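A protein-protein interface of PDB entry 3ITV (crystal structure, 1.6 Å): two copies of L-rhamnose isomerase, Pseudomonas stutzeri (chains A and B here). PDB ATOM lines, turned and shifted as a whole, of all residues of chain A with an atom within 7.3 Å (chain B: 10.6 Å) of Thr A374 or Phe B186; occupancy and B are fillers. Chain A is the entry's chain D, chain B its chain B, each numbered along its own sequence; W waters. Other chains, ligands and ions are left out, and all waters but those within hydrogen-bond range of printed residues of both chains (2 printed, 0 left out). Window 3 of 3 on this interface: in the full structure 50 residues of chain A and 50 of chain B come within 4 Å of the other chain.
Among the printed residues, pairs that only touch across the chains: Leu A304 with Pro B187, Leu A304 with Tyr B228, Leu A361 with Gly B188, Ala A370 with Gln B189, Ala A373 with Gly B188, Ala A373 with Gln B189, Thr A374 with Phe B186, Leu A377 with Pro B187 and Leu A377 with Gly B188.
O of Pro B187 lies within hydrogen-bond range of OG1 of Thr A374 (2.8 Å).
No position is printed for both chains.
Printed residues of chain B within 4 Å of Leu A361: Gly B188 (3.7 Å). Printed residues of chain B within 4 Å of Ala A370: Gln B189 (3.5 Å). No residue of chain B comes within 4 Å of Leu A371. No residue of chain B comes within 4 Å of Glu A375. No residue of chain B comes within 4 Å of Thr A376. Ser B184 touches none of the printed residues of chain A. Phe B186 touches just one residue of chain A: Thr A374. Of the printed residues of chain A, Pro B187 touches Leu A304 (3.9 Å), Thr A374 (2.8 Å) and Leu A377 (3.5 Å). The nearest residue of chain B that does not touch Thr A374 is Gln B189 (4.7 Å). The nearest printed residue of chain B that does not touch Leu A361 is Gln B189 (5.4 Å).
N of Asn B185 lies close to NE2 of Gln B189 (2.8 Å). N of Phe B186 sits close to NE2 of Gln B189. The backbone carbonyl oxygen (O) of Ser B184 sits at hydrogen-bond distance from the backbone NH (N) of Tyr B228 (3.0 Å).
Water W1 lies within hydrogen-bond range of O of Gln B189 (2.9 Å), O of Tyr A364 (3.1 Å), N of Asp A369 (3.3 Å) and N of Ala A370 (3.4 Å). Water W2 lies within hydrogen-bond range of the backbone NH (N) of Ala A370 and the side-chain hydroxyl (OH) of Tyr B143.
Of the 18 printed residues of chain A, 6 touch a printed residue of chain B. Hydrophobic or aromatic side chains of chain A within 4 Å of the printed part of chain B: Leu A304, Leu A361, Ala A370, Ala A373 and Leu A377. Of the 19 printed residues of chain B, 5 touch a printed residue of chain A. Hydrophobic or aromatic side chains of chain B within 4 Å of the printed part of chain A: Phe B186, Pro B187 and Tyr B228. Among the printed residues, no Asp or Glu carboxylate lies within 4 Å of a Lys or Arg side-chain nitrogen of the other chain.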
ATOM      1  N   TYR A 300      14.668  17.731   0.496  1.00  0.00           N
ATOM      2  CA  TYR A 300      16.069  17.751   0.078  1.00  0.00           C
ATOM      3  C   TYR A 300      16.886  18.666   0.987  1.00  0.00           C
ATOM      4  O   TYR A 300      18.012  18.333   1.357  1.00  0.00           O
ATOM      5  CB  TYR A 300      16.195  18.184  -1.389  1.00  0.00           C
ATOM      6  CG  TYR A 300      17.553  17.899  -2.005  1.00  0.00           C
ATOM      7  CD1 TYR A 300      18.207  16.686  -1.771  1.00  0.00           C
ATOM      8  CD2 TYR A 300      18.168  18.826  -2.849  1.00  0.00           C
ATOM      9  CE1 TYR A 300      19.439  16.403  -2.366  1.00  0.00           C
ATOM     10  CE2 TYR A 300      19.401  18.553  -3.449  1.00  0.00           C
ATOM     11  CZ  TYR A 300      20.029  17.339  -3.203  1.00  0.00           C
ATOM     12  OH  TYR A 300      21.241  17.051  -3.795  1.00  0.00           O
ATOM     13  N   PHE A 303      17.891  16.921   3.994  1.00  0.00           N
ATOM     14  CA  PHE A 303      18.990  16.016   3.675  1.00  0.00           C
ATOM     15  C   PHE A 303      20.310  16.791   3.602  1.00  0.00           C
ATOM     16  O   PHE A 303      21.335  16.332   4.106  1.00  0.00           O
ATOM     17  CB  PHE A 303      18.727  15.323   2.333  1.00  0.00           C
ATOM     18  CG  PHE A 303      19.961  14.718   1.706  1.00  0.00           C
ATOM     19  CD1 PHE A 303      20.469  13.505   2.155  1.00  0.00           C
ATOM     20  CD2 PHE A 303      20.623  15.382   0.678  1.00  0.00           C
ATOM     21  CE1 PHE A 303      21.627  12.960   1.587  1.00  0.00           C
ATOM     22  CE2 PHE A 303      21.777  14.851   0.104  1.00  0.00           C
ATOM     23  CZ  PHE A 303      22.281  13.636   0.560  1.00  0.00           C
ATOM     24  N   LEU A 304      20.286  17.969   2.980  1.00  0.00           N
ATOM     25  CA  LEU A 304      21.495  18.773   2.848  1.00  0.00           C
ATOM     26  C   LEU A 304      22.018  19.253   4.202  1.00  0.00           C
ATOM     27  O   LEU A 304      23.221  19.425   4.381  1.00  0.00           O
ATOM     28  CB  LEU A 304      21.245  19.951   1.896  1.00  0.00           C
ATOM     29  CG  LEU A 304      20.959  19.507   0.455  1.00  0.00           C
ATOM     30  CD1 LEU A 304      20.687  20.726  -0.415  1.00  0.00           C
ATOM     31  CD2 LEU A 304      22.144  18.708  -0.091  1.00  0.00           C
ATOM     32  N   LEU A 361      32.727  11.850  -3.552  1.00  0.00           N
ATOM     33  CA  LEU A 361      32.351  13.257  -3.476  1.00  0.00           C
ATOM     34  C   LEU A 361      33.587  14.147  -3.372  1.00  0.00           C
ATOM     35  O   LEU A 361      33.691  15.157  -4.066  1.00  0.00           O
ATOM     36  CB  LEU A 361      31.432  13.506  -2.276  1.00  0.00           C
ATOM     37  CG  LEU A 361      30.924  14.946  -2.122  1.00  0.00           C
ATOM     38  CD1 LEU A 361      30.118  15.354  -3.351  1.00  0.00           C
ATOM     39  CD2 LEU A 361      30.072  15.046  -0.870  1.00  0.00           C
ATOM     40  N   TYR A 364      35.283  14.521  -6.745  1.00  0.00           N
ATOM     41  CA  TYR A 364      34.604  15.411  -7.674  1.00  0.00           C
ATOM     42  C   TYR A 364      34.704  16.863  -7.229  1.00  0.00           C
ATOM     43  O   TYR A 364      34.679  17.773  -8.055  1.00  0.00           O
ATOM     44  CB  TYR A 364      33.135  15.002  -7.833  1.00  0.00           C
ATOM     45  CG  TYR A 364      32.956  13.643  -8.476  1.00  0.00           C
ATOM     46  CD1 TYR A 364      33.601  13.328  -9.675  1.00  0.00           C
ATOM     47  CD2 TYR A 364      32.136  12.677  -7.893  1.00  0.00           C
ATOM     48  CE1 TYR A 364      33.431  12.084 -10.277  1.00  0.00           C
ATOM     49  CE2 TYR A 364      31.958  11.429  -8.488  1.00  0.00           C
ATOM     50  CZ  TYR A 364      32.608  11.141  -9.677  1.00  0.00           C
ATOM     51  OH  TYR A 364      32.432   9.910 -10.269  1.00  0.00           O
ATOM     52  N   ASP A 369      34.221  18.862 -10.660  1.00  0.00           N
ATOM     53  CA  ASP A 369      33.263  18.163 -11.509  1.00  0.00           C
ATOM     54  C   ASP A 369      31.938  18.374 -10.778  1.00  0.00           C
ATOM     55  O   ASP A 369      31.465  17.500 -10.050  1.00  0.00           O
ATOM     56  CB  ASP A 369      33.605  16.674 -11.565  1.00  0.00           C
ATOM     57  CG  ASP A 369      32.779  15.919 -12.586  1.00  0.00           C
ATOM     58  OD1 ASP A 369      31.704  16.417 -12.984  1.00  0.00           O
ATOM     59  OD2 ASP A 369      33.206  14.814 -12.979  1.00  0.00           O
ATOM     60  N   ALA A 370      31.358  19.555 -10.964  1.00  0.00           N
ATOM     61  CA  ALA A 370      30.116  19.926 -10.292  1.00  0.00           C
ATOM     62  C   ALA A 370      28.953  18.980 -10.538  1.00  0.00           C
ATOM     63  O   ALA A 370      28.193  18.669  -9.616  1.00  0.00           O
ATOM     64  CB  ALA A 370      29.719  21.351 -10.682  1.00  0.00           C
ATOM     65  N   LEU A 371      28.808  18.524 -11.779  1.00  0.00           N
ATOM     66  CA  LEU A 371      27.712  17.628 -12.118  1.00  0.00           C
ATOM     67  C   LEU A 371      27.804  16.291 -11.388  1.00  0.00           C
ATOM     68  O   LEU A 371      26.819  15.826 -10.816  1.00  0.00           O
ATOM     69  CB  LEU A 371      27.659  17.404 -13.632  1.00  0.00           C
ATOM     70  CG  LEU A 371      26.509  16.516 -14.111  1.00  0.00           C
ATOM     71  CD1 LEU A 371      25.734  17.222 -15.215  1.00  0.00           C
ATOM     72  CD2 LEU A 371      27.063  15.186 -14.593  1.00  0.00           C
ATOM     73  N   MET A 372      28.979  15.669 -11.396  1.00  0.00           N
ATOM     74  CA  MET A 372      29.123  14.393 -10.706  1.00  0.00           C
ATOM     75  C   MET A 372      29.087  14.575  -9.195  1.00  0.00           C
ATOM     76  O   MET A 372      28.662  13.682  -8.465  1.00  0.00           O
ATOM     77  CB  MET A 372      30.414  13.683 -11.119  1.00  0.00           C
ATOM     78  CG  MET A 372      30.347  13.026 -12.495  1.00  0.00           C
ATOM     79  SD  MET A 372      28.878  11.980 -12.728  1.00  0.00           S
ATOM     80  CE  MET A 372      29.158  10.705 -11.497  1.00  0.00           C
ATOM     81  N   ALA A 373      29.527  15.736  -8.722  1.00  0.00           N
ATOM     82  CA  ALA A 373      29.506  16.000  -7.291  1.00  0.00           C
ATOM     83  C   ALA A 373      28.056  16.032  -6.825  1.00  0.00           C
ATOM     84  O   ALA A 373      27.693  15.386  -5.843  1.00  0.00           O
ATOM     85  CB  ALA A 373      30.180  17.334  -6.987  1.00  0.00           C
ATOM     86  N   THR A 374      27.218  16.774  -7.543  1.00  0.00           N
ATOM     87  CA  THR A 374      25.818  16.872  -7.157  1.00  0.00           C
ATOM     88  C   THR A 374      25.106  15.526  -7.358  1.00  0.00           C
ATOM     89  O   THR A 374      24.242  15.156  -6.563  1.00  0.00           O
ATOM     90  CB  THR A 374      25.112  18.032  -7.932  1.00  0.00           C
ATOM     91  OG1 THR A 374      24.110  18.626  -7.094  1.00  0.00           O
ATOM     92  CG2 THR A 374      24.467  17.536  -9.211  1.00  0.00           C
ATOM     93  N   GLU A 375      25.487  14.784  -8.398  1.00  0.00           N
ATOM     94  CA  GLU A 375      24.884  13.477  -8.657  1.00  0.00           C
ATOM     95  C   GLU A 375      25.277  12.488  -7.555  1.00  0.00           C
ATOM     96  O   GLU A 375      24.532  11.558  -7.246  1.00  0.00           O
ATOM     97  CB  GLU A 375      25.322  12.958 -10.036  1.00  0.00           C
ATOM     98  CG  GLU A 375      24.969  11.500 -10.346  1.00  0.00           C
ATOM     99  CD  GLU A 375      23.476  11.203 -10.326  1.00  0.00           C
ATOM    100  OE1 GLU A 375      22.659  12.147 -10.374  1.00  0.00           O
ATOM    101  OE2 GLU A 375      23.124  10.003 -10.277  1.00  0.00           O
ATOM    102  N   THR A 376      26.444  12.699  -6.951  1.00  0.00           N
ATOM    103  CA  THR A 376      26.895  11.824  -5.876  1.00  0.00           C
ATOM    104  C   THR A 376      25.985  12.022  -4.660  1.00  0.00           C
ATOM    105  O   THR A 376      25.649  11.064  -3.963  1.00  0.00           O
ATOM    106  CB  THR A 376      28.369  12.113  -5.513  1.00  0.00           C
ATOM    107  OG1 THR A 376      29.195  11.817  -6.650  1.00  0.00           O
ATOM    108  CG2 THR A 376      28.818  11.254  -4.339  1.00  0.00           C
ATOM    109  N   LEU A 377      25.584  13.262  -4.403  1.00  0.00           N
ATOM    110  CA  LEU A 377      24.671  13.510  -3.292  1.00  0.00           C
ATOM    111  C   LEU A 377      23.301  12.926  -3.636  1.00  0.00           C
ATOM    112  O   LEU A 377      22.658  12.302  -2.794  1.00  0.00           O
ATOM    113  CB  LEU A 377      24.519  15.007  -3.015  1.00  0.00           C
ATOM    114  CG  LEU A 377      25.687  15.764  -2.381  1.00  0.00           C
ATOM    115  CD1 LEU A 377      25.208  17.162  -2.019  1.00  0.00           C
ATOM    116  CD2 LEU A 377      26.181  15.047  -1.132  1.00  0.00           C
ATOM    117  N   LYS A 378      22.860  13.124  -4.875  1.00  0.00           N
ATOM    118  CA  LYS A 378      21.560  12.613  -5.301  1.00  0.00           C
ATOM    119  C   LYS A 378      21.469  11.092  -5.261  1.00  0.00           C
ATOM    120  O   LYS A 378      20.409  10.539  -4.977  1.00  0.00           O
ATOM    121  CB  LYS A 378      21.216  13.108  -6.710  1.00  0.00           C
ATOM    122  CG  LYS A 378      20.758  14.562  -6.779  1.00  0.00           C
ATOM    123  CD  LYS A 378      19.539  14.810  -5.891  1.00  0.00           C
ATOM    124  CE  LYS A 378      18.864  16.133  -6.226  1.00  0.00           C
ATOM    125  NZ  LYS A 378      18.211  16.101  -7.567  1.00  0.00           N
ATOM    126  N   ARG A 379      22.570  10.405  -5.548  1.00  0.00           N
ATOM    127  CA  ARG A 379      22.536   8.950  -5.514  1.00  0.00           C
ATOM    128  C   ARG A 379      22.180   8.460  -4.115  1.00  0.00           C
ATOM    129  O   ARG A 379      21.533   7.428  -3.956  1.00  0.00           O
ATOM    130  CB  ARG A 379      23.874   8.379  -5.992  1.00  0.00           C
ATOM    131  CG  ARG A 379      24.045   8.568  -7.493  1.00  0.00           C
ATOM    132  CD  ARG A 379      25.381   8.097  -8.031  1.00  0.00           C
ATOM    133  NE  ARG A 379      25.412   8.224  -9.486  1.00  0.00           N
ATOM    134  CZ  ARG A 379      26.474   7.967 -10.245  1.00  0.00           C
ATOM    135  NH1 ARG A 379      27.610   7.568  -9.690  1.00  0.00           N
ATOM    136  NH2 ARG A 379      26.396   8.102 -11.561  1.00  0.00           N
ATOM    137  N   ALA A 380      22.581   9.216  -3.099  1.00  0.00           N
ATOM    138  CA  ALA A 380      22.265   8.851  -1.724  1.00  0.00           C
ATOM    139  C   ALA A 380      20.835   9.287  -1.405  1.00  0.00           C
ATOM    140  O   ALA A 380      20.025   8.505  -0.900  1.00  0.00           O
ATOM    141  CB  ALA A 380      23.248   9.521  -0.765  1.00  0.00           C
ATOM    142  N   ARG A 382      18.293   9.900  -3.379  1.00  0.00           N
ATOM    143  CA  ARG A 382      17.255   9.194  -4.129  1.00  0.00           C
ATOM    144  C   ARG A 382      16.989   7.792  -3.588  1.00  0.00           C
ATOM    145  O   ARG A 382      15.974   7.179  -3.918  1.00  0.00           O
ATOM    146  CB  ARG A 382      17.625   9.082  -5.613  1.00  0.00           C
ATOM    147  CG  ARG A 382      17.674  10.398  -6.379  1.00  0.00           C
ATOM    148  CD  ARG A 382      17.721  10.131  -7.880  1.00  0.00           C
ATOM    149  NE  ARG A 382      18.807   9.226  -8.245  1.00  0.00           N
ATOM    150  CZ  ARG A 382      19.923   9.602  -8.864  1.00  0.00           C
ATOM    151  NH1 ARG A 382      20.105  10.875  -9.198  1.00  0.00           N
ATOM    152  NH2 ARG A 382      20.859   8.706  -9.142  1.00  0.00           N
ATOM    153  N   LYS B 142      36.858  30.201 -13.366  1.00  0.00           N
ATOM    154  CA  LYS B 142      35.550  29.593 -13.578  1.00  0.00           C
ATOM    155  C   LYS B 142      35.020  28.922 -12.311  1.00  0.00           C
ATOM    156  O   LYS B 142      33.858  29.104 -11.949  1.00  0.00           O
ATOM    157  CB  LYS B 142      35.625  28.562 -14.713  1.00  0.00           C
ATOM    158  CG  LYS B 142      34.298  27.888 -15.054  1.00  0.00           C
ATOM    159  CD  LYS B 142      34.434  27.041 -16.320  1.00  0.00           C
ATOM    160  CE  LYS B 142      33.091  26.494 -16.788  1.00  0.00           C
ATOM    161  NZ  LYS B 142      33.202  25.923 -18.167  1.00  0.00           N
ATOM    162  N   TYR B 143      35.875  28.161 -11.633  1.00  0.00           N
ATOM    163  CA  TYR B 143      35.464  27.449 -10.425  1.00  0.00           C
ATOM    164  C   TYR B 143      35.927  28.102  -9.130  1.00  0.00           C
ATOM    165  O   TYR B 143      35.949  27.465  -8.075  1.00  0.00           O
ATOM    166  CB  TYR B 143      35.962  26.002 -10.482  1.00  0.00           C
ATOM    167  CG  TYR B 143      35.453  25.243 -11.686  1.00  0.00           C
ATOM    168  CD1 TYR B 143      34.089  25.019 -11.869  1.00  0.00           C
ATOM    169  CD2 TYR B 143      36.336  24.764 -12.653  1.00  0.00           C
ATOM    170  CE1 TYR B 143      33.615  24.334 -12.989  1.00  0.00           C
ATOM    171  CE2 TYR B 143      35.874  24.079 -13.774  1.00  0.00           C
ATOM    172  CZ  TYR B 143      34.514  23.868 -13.935  1.00  0.00           C
ATOM    173  OH  TYR B 143      34.055  23.194 -15.047  1.00  0.00           O
ATOM    174  N   ASP B 182      33.265  33.535  -5.892  1.00  0.00           N
ATOM    175  CA  ASP B 182      33.473  32.190  -5.355  1.00  0.00           C
ATOM    176  C   ASP B 182      32.279  31.572  -4.652  1.00  0.00           C
ATOM    177  O   ASP B 182      31.710  32.148  -3.721  1.00  0.00           O
ATOM    178  CB  ASP B 182      34.671  32.183  -4.400  1.00  0.00           C
ATOM    179  CG  ASP B 182      35.988  32.361  -5.123  1.00  0.00           C
ATOM    180  OD1 ASP B 182      36.030  33.147  -6.090  1.00  0.00           O
ATOM    181  OD2 ASP B 182      36.983  31.725  -4.715  1.00  0.00           O
ATOM    182  N   GLY B 183      31.919  30.376  -5.104  1.00  0.00           N
ATOM    183  CA  GLY B 183      30.800  29.660  -4.528  1.00  0.00           C
ATOM    184  C   GLY B 183      30.494  28.451  -5.382  1.00  0.00           C
ATOM    185  O   GLY B 183      31.372  27.937  -6.082  1.00  0.00           O
ATOM    186  N   SER B 184      29.246  28.004  -5.340  1.00  0.00           N
ATOM    187  CA  SER B 184      28.831  26.845  -6.114  1.00  0.00           C
ATOM    188  C   SER B 184      27.423  27.036  -6.656  1.00  0.00           C
ATOM    189  O   SER B 184      26.641  27.824  -6.121  1.00  0.00           O
ATOM    190  CB  SER B 184      28.876  25.591  -5.240  1.00  0.00           C
ATOM    191  OG  SER B 184      28.008  25.725  -4.125  1.00  0.00           O
ATOM    192  N   ASN B 185      27.109  26.316  -7.726  1.00  0.00           N
ATOM    193  CA  ASN B 185      25.784  26.378  -8.327  1.00  0.00           C
ATOM    194  C   ASN B 185      24.994  25.106  -8.024  1.00  0.00           C
ATOM    195  O   ASN B 185      23.805  25.026  -8.329  1.00  0.00           O
ATOM    196  CB  ASN B 185      25.887  26.555  -9.847  1.00  0.00           C
ATOM    197  CG  ASN B 185      26.169  27.988 -10.253  1.00  0.00           C
ATOM    198  OD1 ASN B 185      26.427  28.834  -9.401  1.00  0.00           O
ATOM    199  ND2 ASN B 185      26.122  28.266 -11.551  1.00  0.00           N
ATOM    200  N   PHE B 186      25.652  24.122  -7.413  1.00  0.00           N
ATOM    201  CA  PHE B 186      25.010  22.844  -7.106  1.00  0.00           C
ATOM    202  C   PHE B 186      25.391  22.266  -5.757  1.00  0.00           C
ATOM    203  O   PHE B 186      26.547  22.345  -5.346  1.00  0.00           O
ATOM    204  CB  PHE B 186      25.389  21.800  -8.160  1.00  0.00           C
ATOM    205  CG  PHE B 186      24.981  22.170  -9.549  1.00  0.00           C
ATOM    206  CD1 PHE B 186      23.663  22.010  -9.964  1.00  0.00           C
ATOM    207  CD2 PHE B 186      25.904  22.710 -10.434  1.00  0.00           C
ATOM    208  CE1 PHE B 186      23.270  22.385 -11.245  1.00  0.00           C
ATOM    209  CE2 PHE B 186      25.524  23.090 -11.717  1.00  0.00           C
ATOM    210  CZ  PHE B 186      24.204  22.928 -12.124  1.00  0.00           C
ATOM    211  N   PRO B 187      24.420  21.673  -5.048  1.00  0.00           N
ATOM    212  CA  PRO B 187      24.727  21.074  -3.747  1.00  0.00           C
ATOM    213  C   PRO B 187      25.810  20.015  -3.978  1.00  0.00           C
ATOM    214  O   PRO B 187      25.752  19.268  -4.958  1.00  0.00           O
ATOM    215  CB  PRO B 187      23.396  20.453  -3.340  1.00  0.00           C
ATOM    216  CG  PRO B 187      22.398  21.410  -3.922  1.00  0.00           C
ATOM    217  CD  PRO B 187      22.966  21.698  -5.293  1.00  0.00           C
ATOM    218  N   GLY B 188      26.803  19.961  -3.098  1.00  0.00           N
ATOM    219  CA  GLY B 188      27.861  18.977  -3.250  1.00  0.00           C
ATOM    220  C   GLY B 188      29.052  19.448  -4.066  1.00  0.00           C
ATOM    221  O   GLY B 188      30.169  18.968  -3.869  1.00  0.00           O
ATOM    222  N   GLN B 189      28.823  20.386  -4.980  1.00  0.00           N
ATOM    223  CA  GLN B 189      29.906  20.895  -5.818  1.00  0.00           C
ATOM    224  C   GLN B 189      31.085  21.367  -4.971  1.00  0.00           C
ATOM    225  O   GLN B 189      32.243  21.111  -5.305  1.00  0.00           O
ATOM    226  CB  GLN B 189      29.414  22.051  -6.692  1.00  0.00           C
ATOM    227  CG  GLN B 189      30.531  22.749  -7.461  1.00  0.00           C
ATOM    228  CD  GLN B 189      30.045  23.918  -8.303  1.00  0.00           C
ATOM    229  OE1 GLN B 189      30.857  24.637  -8.891  1.00  0.00           O
ATOM    230  NE2 GLN B 189      28.734  24.111  -8.369  1.00  0.00           N
ATOM    231  N   SER B 190      30.779  22.062  -3.879  1.00  0.00           N
ATOM    232  CA  SER B 190      31.804  22.572  -2.977  1.00  0.00           C
ATOM    233  C   SER B 190      31.594  22.027  -1.573  1.00  0.00           C
ATOM    234  O   SER B 190      30.479  21.685  -1.191  1.00  0.00           O
ATOM    235  CB  SER B 190      31.732  24.105  -2.871  1.00  0.00           C
ATOM    236  OG  SER B 190      31.834  24.754  -4.125  1.00  0.00           O
ATOM    237  N   ASN B 191      32.679  21.939  -0.814  1.00  0.00           N
ATOM    238  CA  ASN B 191      32.593  21.542   0.584  1.00  0.00           C
ATOM    239  C   ASN B 191      32.659  22.926   1.234  1.00  0.00           C
ATOM    240  O   ASN B 191      33.695  23.596   1.171  1.00  0.00           O
ATOM    241  CB  ASN B 191      33.799  20.697   1.001  1.00  0.00           C
ATOM    242  CG  ASN B 191      33.745  20.298   2.463  1.00  0.00           C
ATOM    243  OD1 ASN B 191      33.895  21.145   3.342  1.00  0.00           O
ATOM    244  ND2 ASN B 191      33.517  19.015   2.730  1.00  0.00           N
ATOM    245  N   PHE B 192      31.551  23.367   1.825  1.00  0.00           N
ATOM    246  CA  PHE B 192      31.484  24.702   2.421  1.00  0.00           C
ATOM    247  C   PHE B 192      32.661  25.062   3.311  1.00  0.00           C
ATOM    248  O   PHE B 192      33.266  26.125   3.156  1.00  0.00           O
ATOM    249  CB  PHE B 192      30.207  24.884   3.252  1.00  0.00           C
ATOM    250  CG  PHE B 192      28.927  24.655   2.494  1.00  0.00           C
ATOM    251  CD1 PHE B 192      28.799  25.027   1.155  1.00  0.00           C
ATOM    252  CD2 PHE B 192      27.826  24.105   3.146  1.00  0.00           C
ATOM    253  CE1 PHE B 192      27.588  24.855   0.481  1.00  0.00           C
ATOM    254  CE2 PHE B 192      26.612  23.927   2.483  1.00  0.00           C
ATOM    255  CZ  PHE B 192      26.494  24.303   1.146  1.00  0.00           C
ATOM    256  N   PRO B 225      27.526  35.797  -8.824  1.00  0.00           N
ATOM    257  CA  PRO B 225      27.335  34.737  -9.821  1.00  0.00           C
ATOM    258  C   PRO B 225      27.039  33.309  -9.365  1.00  0.00           C
ATOM    259  O   PRO B 225      26.600  32.492 -10.175  1.00  0.00           O
ATOM    260  CB  PRO B 225      28.614  34.821 -10.644  1.00  0.00           C
ATOM    261  CG  PRO B 225      29.632  35.176  -9.606  1.00  0.00           C
ATOM    262  CD  PRO B 225      28.929  36.252  -8.808  1.00  0.00           C
ATOM    263  N   ALA B 226      27.283  32.992  -8.095  1.00  0.00           N
ATOM    264  CA  ALA B 226      27.011  31.640  -7.588  1.00  0.00           C
ATOM    265  C   ALA B 226      25.537  31.549  -7.203  1.00  0.00           C
ATOM    266  O   ALA B 226      25.035  32.386  -6.449  1.00  0.00           O
ATOM    267  CB  ALA B 226      27.894  31.335  -6.386  1.00  0.00           C
ATOM    268  N   PHE B 227      24.851  30.523  -7.705  1.00  0.00           N
ATOM    269  CA  PHE B 227      23.419  30.385  -7.453  1.00  0.00           C
ATOM    270  C   PHE B 227      22.924  29.322  -6.473  1.00  0.00           C
ATOM    271  O   PHE B 227      21.718  29.069  -6.389  1.00  0.00           O
ATOM    272  CB  PHE B 227      22.689  30.260  -8.791  1.00  0.00           C
ATOM    273  CG  PHE B 227      22.871  31.460  -9.676  1.00  0.00           C
ATOM    274  CD1 PHE B 227      22.432  32.716  -9.265  1.00  0.00           C
ATOM    275  CD2 PHE B 227      23.520  31.344 -10.900  1.00  0.00           C
ATOM    276  CE1 PHE B 227      22.641  33.843 -10.063  1.00  0.00           C
ATOM    277  CE2 PHE B 227      23.734  32.463 -11.703  1.00  0.00           C
ATOM    278  CZ  PHE B 227      23.294  33.714 -11.283  1.00  0.00           C
ATOM    279  N   TYR B 228      23.842  28.694  -5.745  1.00  0.00           N
ATOM    280  CA  TYR B 228      23.452  27.741  -4.713  1.00  0.00           C
ATOM    281  C   TYR B 228      24.120  28.188  -3.412  1.00  0.00           C
ATOM    282  O   TYR B 228      23.446  28.393  -2.402  1.00  0.00           O
ATOM    283  CB  TYR B 228      23.860  26.300  -5.034  1.00  0.00           C
ATOM    284  CG  TYR B 228      23.699  25.412  -3.816  1.00  0.00           C
ATOM    285  CD1 TYR B 228      22.450  25.252  -3.199  1.00  0.00           C
ATOM    286  CD2 TYR B 228      24.809  24.831  -3.207  1.00  0.00           C
ATOM    287  CE1 TYR B 228      22.324  24.547  -1.999  1.00  0.00           C
ATOM    288  CE2 TYR B 228      24.693  24.128  -2.015  1.00  0.00           C
ATOM    289  CZ  TYR B 228      23.456  23.994  -1.413  1.00  0.00           C
ATOM    290  OH  TYR B 228      23.364  23.347  -0.202  1.00  0.00           O
ATOM    291  N   SER B 229      25.443  28.333  -3.431  1.00  0.00           N
ATOM    292  CA  SER B 229      26.164  28.795  -2.247  1.00  0.00           C
ATOM    293  C   SER B 229      27.257  29.774  -2.653  1.00  0.00           C
ATOM    294  O   SER B 229      27.766  29.733  -3.773  1.00  0.00           O
ATOM    295  CB  SER B 229      26.791  27.623  -1.472  1.00  0.00           C
ATOM    296  OG  SER B 229      28.091  27.292  -1.945  1.00  0.00           O
ATOM    297  N   THR B 230      27.593  30.670  -1.734  1.00  0.00           N
ATOM    298  CA  THR B 230      28.636  31.664  -1.947  1.00  0.00           C
ATOM    299  C   THR B 230      29.509  31.622  -0.697  1.00  0.00           C
ATOM    300  O   THR B 230      28.991  31.565   0.419  1.00  0.00           O
ATOM    301  CB  THR B 230      28.027  33.076  -2.151  1.00  0.00           C
ATOM    302  OG1 THR B 230      27.339  33.115  -3.409  1.00  0.00           O
ATOM    303  CG2 THR B 230      29.112  34.146  -2.155  1.00  0.00           C
HETATM  304  O   HOH W   1      32.804  20.186  -7.958  1.00  0.00           O
HETATM  305  O   HOH W   2      31.996  21.100 -13.584  1.00  0.00           O
